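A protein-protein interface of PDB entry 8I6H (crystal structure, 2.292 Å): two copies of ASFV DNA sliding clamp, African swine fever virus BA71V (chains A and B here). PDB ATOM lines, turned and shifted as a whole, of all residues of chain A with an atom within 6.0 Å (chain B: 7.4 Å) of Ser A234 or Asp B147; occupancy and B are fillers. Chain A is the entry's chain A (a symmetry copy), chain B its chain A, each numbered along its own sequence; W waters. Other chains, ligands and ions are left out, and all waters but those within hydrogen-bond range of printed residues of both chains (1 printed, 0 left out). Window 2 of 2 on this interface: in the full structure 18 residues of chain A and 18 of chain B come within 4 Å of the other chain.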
ATOM      1  N   MET A 231      -2.375   3.016  20.445  1.00  0.00           N
ATOM      2  CA  MET A 231      -1.108   2.444  20.032  1.00  0.00           C
ATOM      3  C   MET A 231      -1.111   0.939  20.159  1.00  0.00           C
ATOM      4  O   MET A 231      -1.530   0.399  21.165  1.00  0.00           O
ATOM      5  CB  MET A 231       0.032   3.038  20.852  1.00  0.00           C
ATOM      6  CG  MET A 231       1.337   3.100  20.112  1.00  0.00           C
ATOM      7  SD  MET A 231       2.907   3.529  21.233  1.00  0.00           S
ATOM      8  CE  MET A 231       2.308   5.134  22.128  1.00  0.00           C
ATOM      9  N   TYR A 232      -0.640   0.264  19.123  1.00  0.00           N
ATOM     10  CA  TYR A 232      -0.562  -1.189  19.136  1.00  0.00           C
ATOM     11  C   TYR A 232       0.904  -1.566  19.166  1.00  0.00           C
ATOM     12  O   TYR A 232       1.629  -1.346  18.208  1.00  0.00           O
ATOM     13  CB  TYR A 232      -1.289  -1.786  17.921  1.00  0.00           C
ATOM     14  CG  TYR A 232      -2.764  -1.532  17.992  1.00  0.00           C
ATOM     15  CD1 TYR A 232      -3.292  -0.306  17.621  1.00  0.00           C
ATOM     16  CD2 TYR A 232      -3.634  -2.508  18.465  1.00  0.00           C
ATOM     17  CE1 TYR A 232      -4.647  -0.060  17.712  1.00  0.00           C
ATOM     18  CE2 TYR A 232      -4.995  -2.273  18.557  1.00  0.00           C
ATOM     19  CZ  TYR A 232      -5.491  -1.047  18.176  1.00  0.00           C
ATOM     20  OH  TYR A 232      -6.833  -0.791  18.267  1.00  0.00           O
ATOM     21  N   LYS A 233       1.340  -2.106  20.293  1.00  0.00           N
ATOM     22  CA  LYS A 233       2.760  -2.289  20.536  1.00  0.00           C
ATOM     23  C   LYS A 233       3.315  -3.583  19.961  1.00  0.00           C
ATOM     24  O   LYS A 233       4.491  -3.660  19.600  1.00  0.00           O
ATOM     25  CB  LYS A 233       3.041  -2.207  22.032  1.00  0.00           C
ATOM     26  CG  LYS A 233       3.094  -0.771  22.504  1.00  0.00           C
ATOM     27  CD  LYS A 233       3.632  -0.637  23.924  1.00  0.00           C
ATOM     28  CE  LYS A 233       2.572  -1.005  24.960  1.00  0.00           C
ATOM     29  NZ  LYS A 233       3.152  -1.583  26.218  1.00  0.00           N
ATOM     30  N   SER A 234       2.467  -4.589  19.852  1.00  0.00           N
ATOM     31  CA  SER A 234       2.903  -5.869  19.346  1.00  0.00           C
ATOM     32  C   SER A 234       2.175  -6.211  18.058  1.00  0.00           C
ATOM     33  O   SER A 234       0.968  -6.445  18.069  1.00  0.00           O
ATOM     34  CB  SER A 234       2.670  -6.951  20.390  1.00  0.00           C
ATOM     35  OG  SER A 234       2.718  -8.226  19.778  1.00  0.00           O
ATOM     36  N   SER A 235       2.914  -6.237  16.953  1.00  0.00           N
ATOM     37  CA  SER A 235       2.346  -6.486  15.636  1.00  0.00           C
ATOM     38  C   SER A 235       1.743  -7.873  15.489  1.00  0.00           C
ATOM     39  O   SER A 235       0.733  -8.054  14.811  1.00  0.00           O
ATOM     40  CB  SER A 235       3.413  -6.289  14.552  1.00  0.00           C
ATOM     41  OG  SER A 235       3.788  -4.926  14.446  1.00  0.00           O
ATOM     42  N   ASN A 236       2.383  -8.858  16.102  1.00  0.00           N
ATOM     43  CA  ASN A 236       1.961 -10.236  15.945  1.00  0.00           C
ATOM     44  C   ASN A 236       0.610 -10.493  16.610  1.00  0.00           C
ATOM     45  O   ASN A 236      -0.106 -11.410  16.243  1.00  0.00           O
ATOM     46  CB  ASN A 236       3.026 -11.177  16.512  1.00  0.00           C
ATOM     47  N   LYS A 237       0.255  -9.670  17.588  1.00  0.00           N
ATOM     48  CA  LYS A 237      -1.003  -9.861  18.302  1.00  0.00           C
ATOM     49  C   LYS A 237      -2.194  -9.399  17.458  1.00  0.00           C
ATOM     50  O   LYS A 237      -3.327  -9.801  17.712  1.00  0.00           O
ATOM     51  CB  LYS A 237      -0.976  -9.120  19.637  1.00  0.00           C
ATOM     52  CG  LYS A 237       0.031  -9.672  20.646  1.00  0.00           C
ATOM     53  CD  LYS A 237      -0.647 -10.506  21.730  1.00  0.00           C
ATOM     54  CE  LYS A 237       0.323 -10.878  22.852  1.00  0.00           C
ATOM     55  NZ  LYS A 237       0.777  -9.699  23.650  1.00  0.00           N
ATOM     56  N   ILE A 238      -1.942  -8.565  16.449  1.00  0.00           N
ATOM     57  CA  ILE A 238      -3.015  -8.134  15.545  1.00  0.00           C
ATOM     58  C   ILE A 238      -2.718  -8.529  14.096  1.00  0.00           C
ATOM     59  O   ILE A 238      -3.296  -7.986  13.149  1.00  0.00           O
ATOM     60  CB  ILE A 238      -3.267  -6.607  15.628  1.00  0.00           C
ATOM     61  CG1 ILE A 238      -1.995  -5.819  15.299  1.00  0.00           C
ATOM     62  CG2 ILE A 238      -3.789  -6.221  17.017  1.00  0.00           C
ATOM     63  CD1 ILE A 238      -2.240  -4.339  15.083  1.00  0.00           C
ATOM     64  N   ASN A 239      -1.826  -9.500  13.941  1.00  0.00           N
ATOM     65  CA  ASN A 239      -1.427  -9.993  12.627  1.00  0.00           C
ATOM     66  C   ASN A 239      -1.041  -8.893  11.659  1.00  0.00           C
ATOM     67  O   ASN A 239      -1.439  -8.923  10.496  1.00  0.00           O
ATOM     68  CB  ASN A 239      -2.552 -10.825  12.021  1.00  0.00           C
ATOM     69  CG  ASN A 239      -2.300 -12.303  12.151  1.00  0.00           C
ATOM     70  OD1 ASN A 239      -2.413 -12.867  13.246  1.00  0.00           O
ATOM     71  ND2 ASN A 239      -1.983 -12.956  11.026  1.00  0.00           N
ATOM     72  N   THR B 142      -5.008   0.607  29.399  1.00  0.00           N
ATOM     73  CA  THR B 142      -4.255  -0.447  28.736  1.00  0.00           C
ATOM     74  C   THR B 142      -5.113  -1.679  28.511  1.00  0.00           C
ATOM     75  O   THR B 142      -5.835  -2.126  29.403  1.00  0.00           O
ATOM     76  CB  THR B 142      -3.003  -0.829  29.534  1.00  0.00           C
ATOM     77  OG1 THR B 142      -2.200   0.340  29.751  1.00  0.00           O
ATOM     78  CG2 THR B 142      -2.192  -1.856  28.788  1.00  0.00           C
ATOM     79  N   ASP B 143      -5.049  -2.190  27.288  1.00  0.00           N
ATOM     80  CA  ASP B 143      -5.647  -3.465  26.912  1.00  0.00           C
ATOM     81  C   ASP B 143      -4.509  -4.462  26.855  1.00  0.00           C
ATOM     82  O   ASP B 143      -3.598  -4.312  26.042  1.00  0.00           O
ATOM     83  CB  ASP B 143      -6.359  -3.363  25.556  1.00  0.00           C
ATOM     84  CG  ASP B 143      -6.973  -4.687  25.093  1.00  0.00           C
ATOM     85  OD1 ASP B 143      -8.098  -4.653  24.550  1.00  0.00           O
ATOM     86  OD2 ASP B 143      -6.348  -5.760  25.250  1.00  0.00           O
ATOM     87  N   PHE B 144      -4.563  -5.488  27.692  1.00  0.00           N
ATOM     88  CA  PHE B 144      -3.446  -6.412  27.791  1.00  0.00           C
ATOM     89  C   PHE B 144      -3.505  -7.616  26.850  1.00  0.00           C
ATOM     90  O   PHE B 144      -2.491  -8.272  26.639  1.00  0.00           O
ATOM     91  CB  PHE B 144      -3.315  -6.880  29.229  1.00  0.00           C
ATOM     92  CG  PHE B 144      -2.816  -5.818  30.147  1.00  0.00           C
ATOM     93  CD1 PHE B 144      -1.463  -5.513  30.196  1.00  0.00           C
ATOM     94  CD2 PHE B 144      -3.693  -5.103  30.945  1.00  0.00           C
ATOM     95  CE1 PHE B 144      -0.988  -4.521  31.041  1.00  0.00           C
ATOM     96  CE2 PHE B 144      -3.226  -4.108  31.800  1.00  0.00           C
ATOM     97  CZ  PHE B 144      -1.870  -3.818  31.846  1.00  0.00           C
ATOM     98  N   ASP B 145      -4.672  -7.897  26.275  1.00  0.00           N
ATOM     99  CA  ASP B 145      -4.796  -9.000  25.332  1.00  0.00           C
ATOM    100  C   ASP B 145      -4.030  -8.714  24.048  1.00  0.00           C
ATOM    101  O   ASP B 145      -3.496  -9.625  23.420  1.00  0.00           O
ATOM    102  CB  ASP B 145      -6.262  -9.281  24.998  1.00  0.00           C
ATOM    103  CG  ASP B 145      -7.008  -9.951  26.142  1.00  0.00           C
ATOM    104  OD1 ASP B 145      -6.464  -9.997  27.271  1.00  0.00           O
ATOM    105  OD2 ASP B 145      -8.148 -10.419  25.914  1.00  0.00           O
ATOM    106  N   ILE B 146      -3.985  -7.449  23.648  1.00  0.00           N
ATOM    107  CA  ILE B 146      -3.336  -7.109  22.392  1.00  0.00           C
ATOM    108  C   ILE B 146      -2.257  -6.040  22.516  1.00  0.00           C
ATOM    109  O   ILE B 146      -1.869  -5.442  21.514  1.00  0.00           O
ATOM    110  CB  ILE B 146      -4.357  -6.625  21.365  1.00  0.00           C
ATOM    111  CG1 ILE B 146      -5.278  -5.592  22.008  1.00  0.00           C
ATOM    112  CG2 ILE B 146      -5.144  -7.797  20.818  1.00  0.00           C
ATOM    113  CD1 ILE B 146      -6.307  -5.031  21.067  1.00  0.00           C
ATOM    114  N   ASP B 147      -1.769  -5.819  23.734  1.00  0.00           N
ATOM    115  CA  ASP B 147      -0.789  -4.771  23.991  1.00  0.00           C
ATOM    116  C   ASP B 147      -1.228  -3.451  23.371  1.00  0.00           C
ATOM    117  O   ASP B 147      -0.473  -2.824  22.624  1.00  0.00           O
ATOM    118  CB  ASP B 147       0.587  -5.167  23.449  1.00  0.00           C
ATOM    119  CG  ASP B 147       1.214  -6.318  24.218  1.00  0.00           C
ATOM    120  OD1 ASP B 147       0.513  -6.990  25.010  1.00  0.00           O
ATOM    121  OD2 ASP B 147       2.421  -6.560  24.018  1.00  0.00           O
ATOM    122  N   LYS B 148      -2.466  -3.060  23.653  1.00  0.00           N
ATOM    123  CA  LYS B 148      -2.997  -1.808  23.139  1.00  0.00           C
ATOM    124  C   LYS B 148      -3.003  -0.764  24.234  1.00  0.00           C
ATOM    125  O   LYS B 148      -3.375  -1.048  25.376  1.00  0.00           O
ATOM    126  CB  LYS B 148      -4.413  -1.982  22.572  1.00  0.00           C
ATOM    127  CG  LYS B 148      -5.004  -0.662  22.082  1.00  0.00           C
ATOM    128  CD  LYS B 148      -6.383  -0.810  21.440  1.00  0.00           C
ATOM    129  CE  LYS B 148      -7.489  -0.958  22.447  1.00  0.00           C
ATOM    130  NZ  LYS B 148      -8.821  -0.779  21.771  1.00  0.00           N
ATOM    131  N   GLU B 149      -2.590   0.446  23.879  1.00  0.00           N
ATOM    132  CA  GLU B 149      -2.510   1.542  24.827  1.00  0.00           C
ATOM    133  C   GLU B 149      -3.249   2.739  24.272  1.00  0.00           C
ATOM    134  O   GLU B 149      -2.904   3.253  23.211  1.00  0.00           O
ATOM    135  CB  GLU B 149      -1.056   1.894  25.104  1.00  0.00           C
ATOM    136  CG  GLU B 149      -0.795   2.406  26.486  1.00  0.00           C
ATOM    137  CD  GLU B 149       0.694   2.472  26.793  1.00  0.00           C
ATOM    138  OE1 GLU B 149       1.259   3.587  26.749  1.00  0.00           O
ATOM    139  OE2 GLU B 149       1.294   1.403  27.063  1.00  0.00           O
HETATM  140  O   HOH W   1      -0.503  -4.551  19.495  1.00  0.00           O
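Of the printed residues of chain B, Met A231 touches Asp B147, Lys B148 and Glu B149.
Of the printed residues of chain B, Tyr A232 touches Ile B146, Asp B147 and Lys B148.
Ser A234 touches one residue of chain B.
Asp B143 touches none of the printed residues of chain A.
Of the printed residues of chain A, Ile B146 touches Tyr A232.
Of the printed residues of chain A, Asp B147 touches Met A231, Tyr A232, Lys A233, Ser A234 and Lys A237.
Printed residues of chain A within 4 Å of Lys B148: Met A231 and Tyr A232.
OD2 of Asp B143 lies within hydrogen-bond range of N of Ile B146 (3.3 Å).
The side-chain carboxylate of Asp B143 is in hydrogen-bond range of the backbone NH of Asp B145, 2.9 Å away.
The backbone carbonyl oxygen (O) of Lys B148 is in hydrogen-bond range of the backbone NH (N) of Asp B143 (2.8 Å).
No position is printed for both chains.
Among the printed residues, merely in contact across the chains: Tyr A232 with Lys B148, Met A231 with Lys B148, Lys A237 with Asp B145, Ser A234 with Asp B147, Met A231 with Asp B147, Tyr A232 with Asp B147 and Tyr A232 with Ile B146.
The backbone carbonyl oxygen (O) of Glu B149 lies within hydrogen-bond range of the backbone NH (N) of Met A231, at 2.8 Å.
NZ of Lys A237 is in salt-bridge range of OD1 of Asp B147 (3.0 Å).
OE2 of Glu B149 is in salt-bridge range of NZ of Lys A233 (3.6 Å).
The backbone NH (N) of Lys A233 is in hydrogen-bond range of the backbone carbonyl oxygen (O) of Asp B147 (3.0 Å).
Water W1 lies within hydrogen-bond range of the backbone carbonyl oxygen of Ile B146 (2.6 Å), the backbone carbonyl oxygen of Ser A234 (2.8 Å) and the backbone NH of Lys A233 (3.2 Å).
Printed residues of chain B that touch a printed residue of chain A: Asp B145, Ile B146, Asp B147, Lys B148 and Glu B149.
Of the 9 printed residues of chain A, 5 touch a printed residue of chain B.
Hydrophobic or aromatic side chains of chain A within 4 Å of the printed part of chain B: Met A231 and Tyr A232.
Along chain A the printed residues that touch a printed residue of chain B span positions 231 to 237.
Among the printed residues, Asp or Glu carboxylates within 4 Å of a Lys or Arg side-chain nitrogen of the other chain: Lys A233 with Glu B149 (3.6 Å) and Lys A237 with Asp B147 (3.0 Å).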
